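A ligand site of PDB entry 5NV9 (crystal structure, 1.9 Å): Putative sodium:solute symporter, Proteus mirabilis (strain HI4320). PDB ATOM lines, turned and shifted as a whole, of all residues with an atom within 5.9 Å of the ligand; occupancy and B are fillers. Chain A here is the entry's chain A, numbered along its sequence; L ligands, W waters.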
ATOM      1  N   PHE A  55       7.301 -33.586 -13.625  1.00  0.00           N
ATOM      2  CA  PHE A  55       5.995 -33.473 -12.910  1.00  0.00           C
ATOM      3  C   PHE A  55       6.031 -32.325 -11.899  1.00  0.00           C
ATOM      4  O   PHE A  55       5.104 -31.516 -11.850  1.00  0.00           O
ATOM      5  CB  PHE A  55       5.610 -34.823 -12.266  1.00  0.00           C
ATOM      6  CG  PHE A  55       4.289 -34.819 -11.503  1.00  0.00           C
ATOM      7  CD1 PHE A  55       3.099 -34.757 -12.188  1.00  0.00           C
ATOM      8  CD2 PHE A  55       4.252 -34.913 -10.102  1.00  0.00           C
ATOM      9  CE1 PHE A  55       1.898 -34.761 -11.520  1.00  0.00           C
ATOM     10  CE2 PHE A  55       3.054 -34.921  -9.425  1.00  0.00           C
ATOM     11  CZ  PHE A  55       1.877 -34.857 -10.135  1.00  0.00           C
ATOM     12  N   THR A  57       8.145 -29.704 -11.737  1.00  0.00           N
ATOM     13  CA  THR A  57       8.329 -28.450 -12.519  1.00  0.00           C
ATOM     14  C   THR A  57       6.935 -27.953 -12.983  1.00  0.00           C
ATOM     15  O   THR A  57       6.639 -26.817 -12.776  1.00  0.00           O
ATOM     16  CB  THR A  57       9.307 -28.668 -13.733  1.00  0.00           C
ATOM     17  OG1 THR A  57      10.635 -28.946 -13.256  1.00  0.00           O
ATOM     18  CG2 THR A  57       9.381 -27.447 -14.753  1.00  0.00           C
ATOM     19  N   THR A  58       6.090 -28.810 -13.552  1.00  0.00           N
ATOM     20  CA  THR A  58       4.804 -28.327 -14.135  1.00  0.00           C
ATOM     21  C   THR A  58       3.738 -28.052 -13.082  1.00  0.00           C
ATOM     22  O   THR A  58       2.961 -27.116 -13.223  1.00  0.00           O
ATOM     23  CB  THR A  58       4.220 -29.309 -15.185  1.00  0.00           C
ATOM     24  OG1 THR A  58       4.051 -30.589 -14.568  1.00  0.00           O
ATOM     25  CG2 THR A  58       5.131 -29.456 -16.383  1.00  0.00           C
ATOM     26  N   LEU A  59       3.743 -28.837 -12.007  1.00  0.00           N
ATOM     27  CA  LEU A  59       2.719 -28.757 -10.961  1.00  0.00           C
ATOM     28  C   LEU A  59       3.188 -27.873  -9.838  1.00  0.00           C
ATOM     29  O   LEU A  59       4.053 -28.273  -9.064  1.00  0.00           O
ATOM     30  CB  LEU A  59       2.401 -30.126 -10.363  1.00  0.00           C
ATOM     31  CG  LEU A  59       1.065 -30.235  -9.633  1.00  0.00           C
ATOM     32  CD1 LEU A  59       0.607 -31.693  -9.514  1.00  0.00           C
ATOM     33  CD2 LEU A  59       1.124 -29.591  -8.274  1.00  0.00           C
ATOM     34  N   SER A  60       2.539 -26.734  -9.702  1.00  0.00           N
ATOM     35  CA  SER A  60       2.951 -25.667  -8.792  1.00  0.00           C
ATOM     36  C   SER A  60       1.849 -25.395  -7.768  1.00  0.00           C
ATOM     37  O   SER A  60       0.869 -26.142  -7.670  1.00  0.00           O
ATOM     38  CB  SER A  60       3.290 -24.431  -9.602  1.00  0.00           C
ATOM     39  OG  SER A  60       2.164 -23.660  -9.948  1.00  0.00           O
ATOM     40  N   SER A  61       1.982 -24.322  -7.010  1.00  0.00           N
ATOM     41  CA  SER A  61       0.897 -23.907  -6.120  1.00  0.00           C
ATOM     42  C   SER A  61      -0.375 -23.514  -6.833  1.00  0.00           C
ATOM     43  O   SER A  61      -1.424 -23.460  -6.220  1.00  0.00           O
ATOM     44  CB  SER A  61       1.413 -22.772  -5.251  1.00  0.00           C
ATOM     45  OG  SER A  61       1.711 -21.683  -6.096  1.00  0.00           O
ATOM     46  N   ILE A  62      -0.298 -23.249  -8.139  1.00  0.00           N
ATOM     47  CA  ILE A  62      -1.454 -23.028  -8.988  1.00  0.00           C
ATOM     48  C   ILE A  62      -2.372 -24.274  -8.992  1.00  0.00           C
ATOM     49  O   ILE A  62      -3.562 -24.163  -8.701  1.00  0.00           O
ATOM     50  CB  ILE A  62      -1.014 -22.714 -10.450  1.00  0.00           C
ATOM     51  CG1 ILE A  62      -0.355 -21.346 -10.551  1.00  0.00           C
ATOM     52  CG2 ILE A  62      -2.193 -22.784 -11.425  1.00  0.00           C
ATOM     53  CD1 ILE A  62       0.352 -21.132 -11.853  1.00  0.00           C
ATOM     54  N   THR A  63      -1.822 -25.436  -9.317  1.00  0.00           N
ATOM     55  CA  THR A  63      -2.592 -26.677  -9.278  1.00  0.00           C
ATOM     56  C   THR A  63      -3.008 -26.973  -7.833  1.00  0.00           C
ATOM     57  O   THR A  63      -4.179 -27.343  -7.569  1.00  0.00           O
ATOM     58  CB  THR A  63      -1.779 -27.894  -9.841  1.00  0.00           C
ATOM     59  OG1 THR A  63      -1.793 -27.894 -11.270  1.00  0.00           O
ATOM     60  CG2 THR A  63      -2.295 -29.257  -9.306  1.00  0.00           C
ATOM     61  N   PHE A  64      -2.060 -26.812  -6.894  1.00  0.00           N
ATOM     62  CA  PHE A  64      -2.255 -27.306  -5.525  1.00  0.00           C
ATOM     63  C   PHE A  64      -3.464 -26.617  -4.880  1.00  0.00           C
ATOM     64  O   PHE A  64      -4.285 -27.287  -4.244  1.00  0.00           O
ATOM     65  CB  PHE A  64      -1.004 -27.120  -4.663  1.00  0.00           C
ATOM     66  CG  PHE A  64      -0.921 -28.046  -3.448  1.00  0.00           C
ATOM     67  CD1 PHE A  64      -1.777 -27.906  -2.367  1.00  0.00           C
ATOM     68  CD2 PHE A  64       0.064 -29.024  -3.379  1.00  0.00           C
ATOM     69  CE1 PHE A  64      -1.696 -28.784  -1.264  1.00  0.00           C
ATOM     70  CE2 PHE A  64       0.187 -29.893  -2.268  1.00  0.00           C
ATOM     71  CZ  PHE A  64      -0.681 -29.765  -1.203  1.00  0.00           C
ATOM     72  N   ILE A  67      -6.993 -26.305  -8.182  1.00  0.00           N
ATOM     73  CA  ILE A  67      -7.728 -27.443  -8.703  1.00  0.00           C
ATOM     74  C   ILE A  67      -8.746 -27.892  -7.639  1.00  0.00           C
ATOM     75  O   ILE A  67      -9.943 -28.045  -7.977  1.00  0.00           O
ATOM     76  CB  ILE A  67      -6.871 -28.615  -9.204  1.00  0.00           C
ATOM     77  CG1 ILE A  67      -6.255 -28.356 -10.603  1.00  0.00           C
ATOM     78  CG2 ILE A  67      -7.681 -29.893  -9.223  1.00  0.00           C
ATOM     79  CD1 ILE A  67      -7.210 -27.854 -11.673  1.00  0.00           C
ATOM     80  N   PHE A  78     -12.047 -30.257 -15.933  1.00  0.00           N
ATOM     81  CA  PHE A  78     -10.673 -29.913 -16.214  1.00  0.00           C
ATOM     82  C   PHE A  78      -9.656 -31.056 -16.181  1.00  0.00           C
ATOM     83  O   PHE A  78      -8.617 -30.971 -16.787  1.00  0.00           O
ATOM     84  CB  PHE A  78     -10.191 -28.830 -15.263  1.00  0.00           C
ATOM     85  CG  PHE A  78     -10.518 -27.421 -15.697  1.00  0.00           C
ATOM     86  CD1 PHE A  78     -11.817 -27.074 -16.143  1.00  0.00           C
ATOM     87  CD2 PHE A  78      -9.579 -26.413 -15.536  1.00  0.00           C
ATOM     88  CE1 PHE A  78     -12.125 -25.764 -16.484  1.00  0.00           C
ATOM     89  CE2 PHE A  78      -9.874 -25.097 -15.910  1.00  0.00           C
ATOM     90  CZ  PHE A  78     -11.152 -24.769 -16.370  1.00  0.00           C
ATOM     91  N   GLY A  81      -7.778 -32.317 -19.061  1.00  0.00           N
ATOM     92  CA  GLY A  81      -6.453 -31.737 -19.277  1.00  0.00           C
ATOM     93  C   GLY A  81      -5.252 -32.597 -18.969  1.00  0.00           C
ATOM     94  O   GLY A  81      -4.290 -32.599 -19.733  1.00  0.00           O
ATOM     95  N   GLN A  82      -5.300 -33.313 -17.836  1.00  0.00           N
ATOM     96  CA  GLN A  82      -4.231 -34.198 -17.402  1.00  0.00           C
ATOM     97  C   GLN A  82      -3.994 -35.380 -18.332  1.00  0.00           C
ATOM     98  O   GLN A  82      -2.853 -35.765 -18.633  1.00  0.00           O
ATOM     99  CB  GLN A  82      -4.542 -34.767 -15.983  1.00  0.00           C
ATOM    100  CG  GLN A  82      -4.930 -33.691 -15.000  1.00  0.00           C
ATOM    101  CD  GLN A  82      -3.748 -32.822 -14.613  1.00  0.00           C
ATOM    102  OE1 GLN A  82      -2.601 -33.242 -14.693  1.00  0.00           O
ATOM    103  NE2 GLN A  82      -4.040 -31.665 -14.076  1.00  0.00           N
ATOM    104  N   ALA A  85      -2.358 -34.567 -21.553  1.00  0.00           N
ATOM    105  CA  ALA A  85      -0.936 -34.266 -21.327  1.00  0.00           C
ATOM    106  C   ALA A  85      -0.166 -35.565 -21.399  1.00  0.00           C
ATOM    107  O   ALA A  85       1.011 -35.573 -21.771  1.00  0.00           O
ATOM    108  CB  ALA A  85      -0.725 -33.609 -19.978  1.00  0.00           C
ATOM    109  N   ARG A 135       5.690 -16.300 -14.299  1.00  0.00           N
ATOM    110  CA  ARG A 135       5.183 -17.509 -13.673  1.00  0.00           C
ATOM    111  C   ARG A 135       5.713 -17.646 -12.229  1.00  0.00           C
ATOM    112  O   ARG A 135       4.939 -18.025 -11.322  1.00  0.00           O
ATOM    113  CB  ARG A 135       5.483 -18.762 -14.549  1.00  0.00           C
ATOM    114  CG  ARG A 135       5.179 -20.109 -13.908  1.00  0.00           C
ATOM    115  CD  ARG A 135       5.534 -21.220 -14.880  1.00  0.00           C
ATOM    116  NE  ARG A 135       5.640 -22.544 -14.280  1.00  0.00           N
ATOM    117  CZ  ARG A 135       4.625 -23.262 -13.874  1.00  0.00           C
ATOM    118  NH1 ARG A 135       3.375 -22.786 -14.020  1.00  0.00           N
ATOM    119  NH2 ARG A 135       4.835 -24.475 -13.303  1.00  0.00           N
ATOM    120  N   ILE A 139       3.465 -17.651  -8.926  1.00  0.00           N
ATOM    121  CA  ILE A 139       3.494 -18.848  -8.107  1.00  0.00           C
ATOM    122  C   ILE A 139       3.734 -18.389  -6.650  1.00  0.00           C
ATOM    123  O   ILE A 139       3.159 -18.914  -5.732  1.00  0.00           O
ATOM    124  CB  ILE A 139       4.579 -19.853  -8.530  1.00  0.00           C
ATOM    125  CG1 ILE A 139       4.074 -20.672  -9.726  1.00  0.00           C
ATOM    126  CG2 ILE A 139       4.882 -20.813  -7.396  1.00  0.00           C
ATOM    127  CD1 ILE A 139       5.172 -21.477 -10.412  1.00  0.00           C
ATOM    128  N   PHE A 243      -6.636 -27.283 -23.518  1.00  0.00           N
ATOM    129  CA  PHE A 243      -5.581 -28.052 -22.837  1.00  0.00           C
ATOM    130  C   PHE A 243      -4.652 -28.828 -23.796  1.00  0.00           C
ATOM    131  O   PHE A 243      -3.433 -28.942 -23.499  1.00  0.00           O
ATOM    132  CB  PHE A 243      -6.119 -29.000 -21.758  1.00  0.00           C
ATOM    133  CG  PHE A 243      -6.388 -28.313 -20.452  1.00  0.00           C
ATOM    134  CD1 PHE A 243      -5.453 -27.482 -19.891  1.00  0.00           C
ATOM    135  CD2 PHE A 243      -7.607 -28.420 -19.835  1.00  0.00           C
ATOM    136  CE1 PHE A 243      -5.696 -26.809 -18.678  1.00  0.00           C
ATOM    137  CE2 PHE A 243      -7.861 -27.759 -18.638  1.00  0.00           C
ATOM    138  CZ  PHE A 243      -6.902 -26.954 -18.049  1.00  0.00           C
ATOM    139  N   ASN A 247      -0.775 -28.104 -23.438  1.00  0.00           N
ATOM    140  CA  ASN A 247       0.054 -29.256 -23.145  1.00  0.00           C
ATOM    141  C   ASN A 247       1.123 -29.386 -24.226  1.00  0.00           C
ATOM    142  O   ASN A 247       2.272 -29.668 -23.901  1.00  0.00           O
ATOM    143  CB  ASN A 247      -0.766 -30.590 -23.019  1.00  0.00           C
ATOM    144  CG  ASN A 247      -1.625 -30.638 -21.750  1.00  0.00           C
ATOM    145  OD1 ASN A 247      -1.289 -30.032 -20.750  1.00  0.00           O
ATOM    146  ND2 ASN A 247      -2.766 -31.309 -21.812  1.00  0.00           N
ATOM    147  N   GLN A 250       3.621 -26.907 -23.316  1.00  0.00           N
ATOM    148  CA  GLN A 250       4.399 -27.303 -22.077  1.00  0.00           C
ATOM    149  C   GLN A 250       5.493 -28.329 -22.374  1.00  0.00           C
ATOM    150  O   GLN A 250       6.600 -28.192 -21.901  1.00  0.00           O
ATOM    151  CB  GLN A 250       3.455 -27.837 -21.003  1.00  0.00           C
ATOM    152  CG  GLN A 250       4.074 -28.243 -19.660  1.00  0.00           C
ATOM    153  CD  GLN A 250       4.681 -27.074 -18.916  1.00  0.00           C
ATOM    154  OE1 GLN A 250       4.043 -26.478 -18.025  1.00  0.00           O
ATOM    155  NE2 GLN A 250       5.912 -26.708 -19.285  1.00  0.00           N
ATOM    156  N   PHE A 251       5.171 -29.308 -23.209  1.00  0.00           N
ATOM    157  CA  PHE A 251       6.042 -30.424 -23.477  1.00  0.00           C
ATOM    158  C   PHE A 251       6.915 -30.374 -24.713  1.00  0.00           C
ATOM    159  O   PHE A 251       7.812 -31.229 -24.815  1.00  0.00           O
ATOM    160  CB  PHE A 251       5.224 -31.743 -23.390  1.00  0.00           C
ATOM    161  CG  PHE A 251       4.718 -31.996 -22.009  1.00  0.00           C
ATOM    162  CD1 PHE A 251       5.512 -32.647 -21.067  1.00  0.00           C
ATOM    163  CD2 PHE A 251       3.465 -31.514 -21.602  1.00  0.00           C
ATOM    164  CE1 PHE A 251       5.067 -32.840 -19.769  1.00  0.00           C
ATOM    165  CE2 PHE A 251       3.004 -31.705 -20.288  1.00  0.00           C
ATOM    166  CZ  PHE A 251       3.820 -32.377 -19.385  1.00  0.00           C
ATOM    167  N   VAL A 281       1.114 -38.179 -13.483  1.00  0.00           N
ATOM    168  CA  VAL A 281       0.059 -37.356 -13.965  1.00  0.00           C
ATOM    169  C   VAL A 281      -1.247 -38.180 -14.019  1.00  0.00           C
ATOM    170  O   VAL A 281      -2.340 -37.649 -13.867  1.00  0.00           O
ATOM    171  CB  VAL A 281       0.446 -36.750 -15.344  1.00  0.00           C
ATOM    172  CG1 VAL A 281      -0.725 -36.010 -15.939  1.00  0.00           C
ATOM    173  CG2 VAL A 281       1.628 -35.797 -15.188  1.00  0.00           C
ATOM    174  N   PRO A 285      -2.972 -35.867  -9.798  1.00  0.00           N
ATOM    175  CA  PRO A 285      -4.002 -34.847 -10.020  1.00  0.00           C
ATOM    176  C   PRO A 285      -5.385 -35.248  -9.619  1.00  0.00           C
ATOM    177  O   PRO A 285      -6.151 -34.414  -9.117  1.00  0.00           O
ATOM    178  CB  PRO A 285      -3.937 -34.617 -11.549  1.00  0.00           C
ATOM    179  CG  PRO A 285      -2.473 -34.765 -11.785  1.00  0.00           C
ATOM    180  CD  PRO A 285      -2.081 -35.955 -10.961  1.00  0.00           C
ATOM    181  N   SER A 343       8.759 -25.575  -8.874  1.00  0.00           N
ATOM    182  CA  SER A 343       8.422 -24.850 -10.136  1.00  0.00           C
ATOM    183  C   SER A 343       9.282 -23.592 -10.286  1.00  0.00           C
ATOM    184  O   SER A 343       9.816 -23.327 -11.380  1.00  0.00           O
ATOM    185  CB  SER A 343       6.912 -24.505 -10.132  1.00  0.00           C
ATOM    186  OG  SER A 343       6.153 -25.718 -10.263  1.00  0.00           O
HETATM  187  C1  LIG L   1       0.618 -25.620 -12.526  1.00  0.00           C
HETATM  188  C2  LIG L   1       0.231 -26.177 -13.870  1.00  0.00           C
HETATM  189  C3  LIG L   1      -0.977 -25.434 -14.388  1.00  0.00           C
HETATM  190  C4  LIG L   1      -1.570 -26.083 -15.661  1.00  0.00           C
HETATM  191  C5  LIG L   1      -1.942 -27.498 -15.261  1.00  0.00           C
HETATM  192  C6  LIG L   1      -0.695 -28.244 -14.729  1.00  0.00           C
HETATM  193  C7  LIG L   1      -0.953 -29.689 -14.273  1.00  0.00           C
HETATM  194  C8  LIG L   1       0.305 -30.335 -13.760  1.00  0.00           C
HETATM  195  C9  LIG L   1       0.096 -31.817 -13.459  1.00  0.00           C
HETATM  196  C10 LIG L   1      -3.754 -28.757 -16.366  1.00  0.00           C
HETATM  197  C11 LIG L   1      -4.006 -29.750 -17.472  1.00  0.00           C
HETATM  198  N1  LIG L   1      -2.517 -28.241 -16.393  1.00  0.00           N
HETATM  199  O1  LIG L   1       0.145 -26.183 -11.486  1.00  0.00           O
HETATM  200  O2  LIG L   1       1.356 -24.573 -12.501  1.00  0.00           O
HETATM  201  O3  LIG L   1       1.332 -26.085 -14.816  1.00  0.00           O
HETATM  202  O4  LIG L   1      -2.771 -25.361 -16.111  1.00  0.00           O
HETATM  203  O5  LIG L   1      -0.149 -27.550 -13.617  1.00  0.00           O
HETATM  204  O6  LIG L   1      -1.895 -29.719 -13.198  1.00  0.00           O
HETATM  205  O7  LIG L   1       1.359 -30.192 -14.705  1.00  0.00           O
HETATM  206  O8  LIG L   1      -0.195 -32.589 -14.659  1.00  0.00           O
HETATM  207  O9  LIG L   1      -4.590 -28.505 -15.493  1.00  0.00           O
HETATM  208  O   HOH W   1       1.144 -30.162 -17.341  1.00  0.00           O
HETATM  209  O   HOH W   2      -4.972 -25.868 -14.594  1.00  0.00           O
HETATM  210  O   HOH W   3      -6.571 -30.096 -14.737  1.00  0.00           O
HETATM  211  O   HOH W   4       1.367 -32.821 -16.986  1.00  0.00           O
HETATM  212  O   HOH W   5       2.053 -24.834 -17.293  1.00  0.00           O
HETATM  213  O   HOH W   6      -0.920 -28.365 -19.000  1.00  0.00           O
HETATM  214  O   HOH W   7      -2.571 -25.387 -18.694  1.00  0.00           O
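OE1 of Gln 82 lies within hydrogen-bond range of O8 of the ligand (2.5 Å). O of Thr 58 lies within hydrogen-bond range of O3 of the ligand, at 2.5 Å. O7 of the ligand is in hydrogen-bond range of OG1 of Thr 58, 2.7 Å away. O1 of the ligand sits at hydrogen-bond distance from N of Thr 63 (3.0 Å). An oxygen (O1) of the ligand lies within hydrogen-bond range of the side-chain hydroxyl of Thr 63, at 2.6 Å. N of Ser 60 lies within hydrogen-bond range of O1 of the ligand (3.0 Å). The side-chain hydroxyl of Ser 60 is in hydrogen-bond range of an oxygen (O2) of the ligand (2.8 Å). An oxygen (O2) of the ligand lies within salt-bridge range of the guanidinium group (NH1) of Arg 135 (3.1 Å).
The backbone carbonyl oxygen (O) of Thr 58 sits at hydrogen-bond distance from the guanidinium group (NH2) of Arg 135 (3.2 Å). The side-chain hydroxyl of Thr 58 sits at hydrogen-bond distance from the backbone carbonyl oxygen of Phe 55 (3.1 Å). The side-chain hydroxyl (OG) of Ser 60 sits close to the backbone NH (N) of Ile 62 (3.1 Å). The guanidinium group of Arg 135 lies within hydrogen-bond range of the backbone carbonyl oxygen of Thr 57 (3.0 Å). O of Gly 81 lies within hydrogen-bond range of ND2 of Asn 247. The backbone carbonyl oxygen of Phe 243 sits at hydrogen-bond distance from the side-chain amide nitrogen of Asn 247, at 3.0 Å.
Residues that only touch the ligand: Gly 81 (3.4 Å), Phe 243 (3.6 Å), Ile 62 (3.6 Å), Leu 59 (3.7 Å), Val 281 (3.7 Å) and Phe 55 (3.96 Å). Hydrophobic or aromatic side chains that line the ligand: Phe 55, Leu 59, Ile 62, Phe 243 and Val 281. Within 4 Å of the ligand: Phe 55, Thr 58, Leu 59, Ser 60, Ile 62, Thr 63, Gly 81, Gln 82, Arg 135, Phe 243 and Val 281.
Water W3 lies within hydrogen-bond range of an oxygen (O9) of the ligand (2.7 Å), the backbone carbonyl oxygen of Phe 78 (3.0 Å) and the side-chain amide nitrogen of Gln 82 (3.1 Å). Water W5 lies within hydrogen-bond range of OE1 of Gln 250 (2.7 Å) and O3 of the ligand (2.9 Å). Water W6 lies within hydrogen-bond range of the side-chain amide oxygen (OD1) of Asn 247 (2.4 Å) and a nitrogen (N1) of the ligand (3.1 Å).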
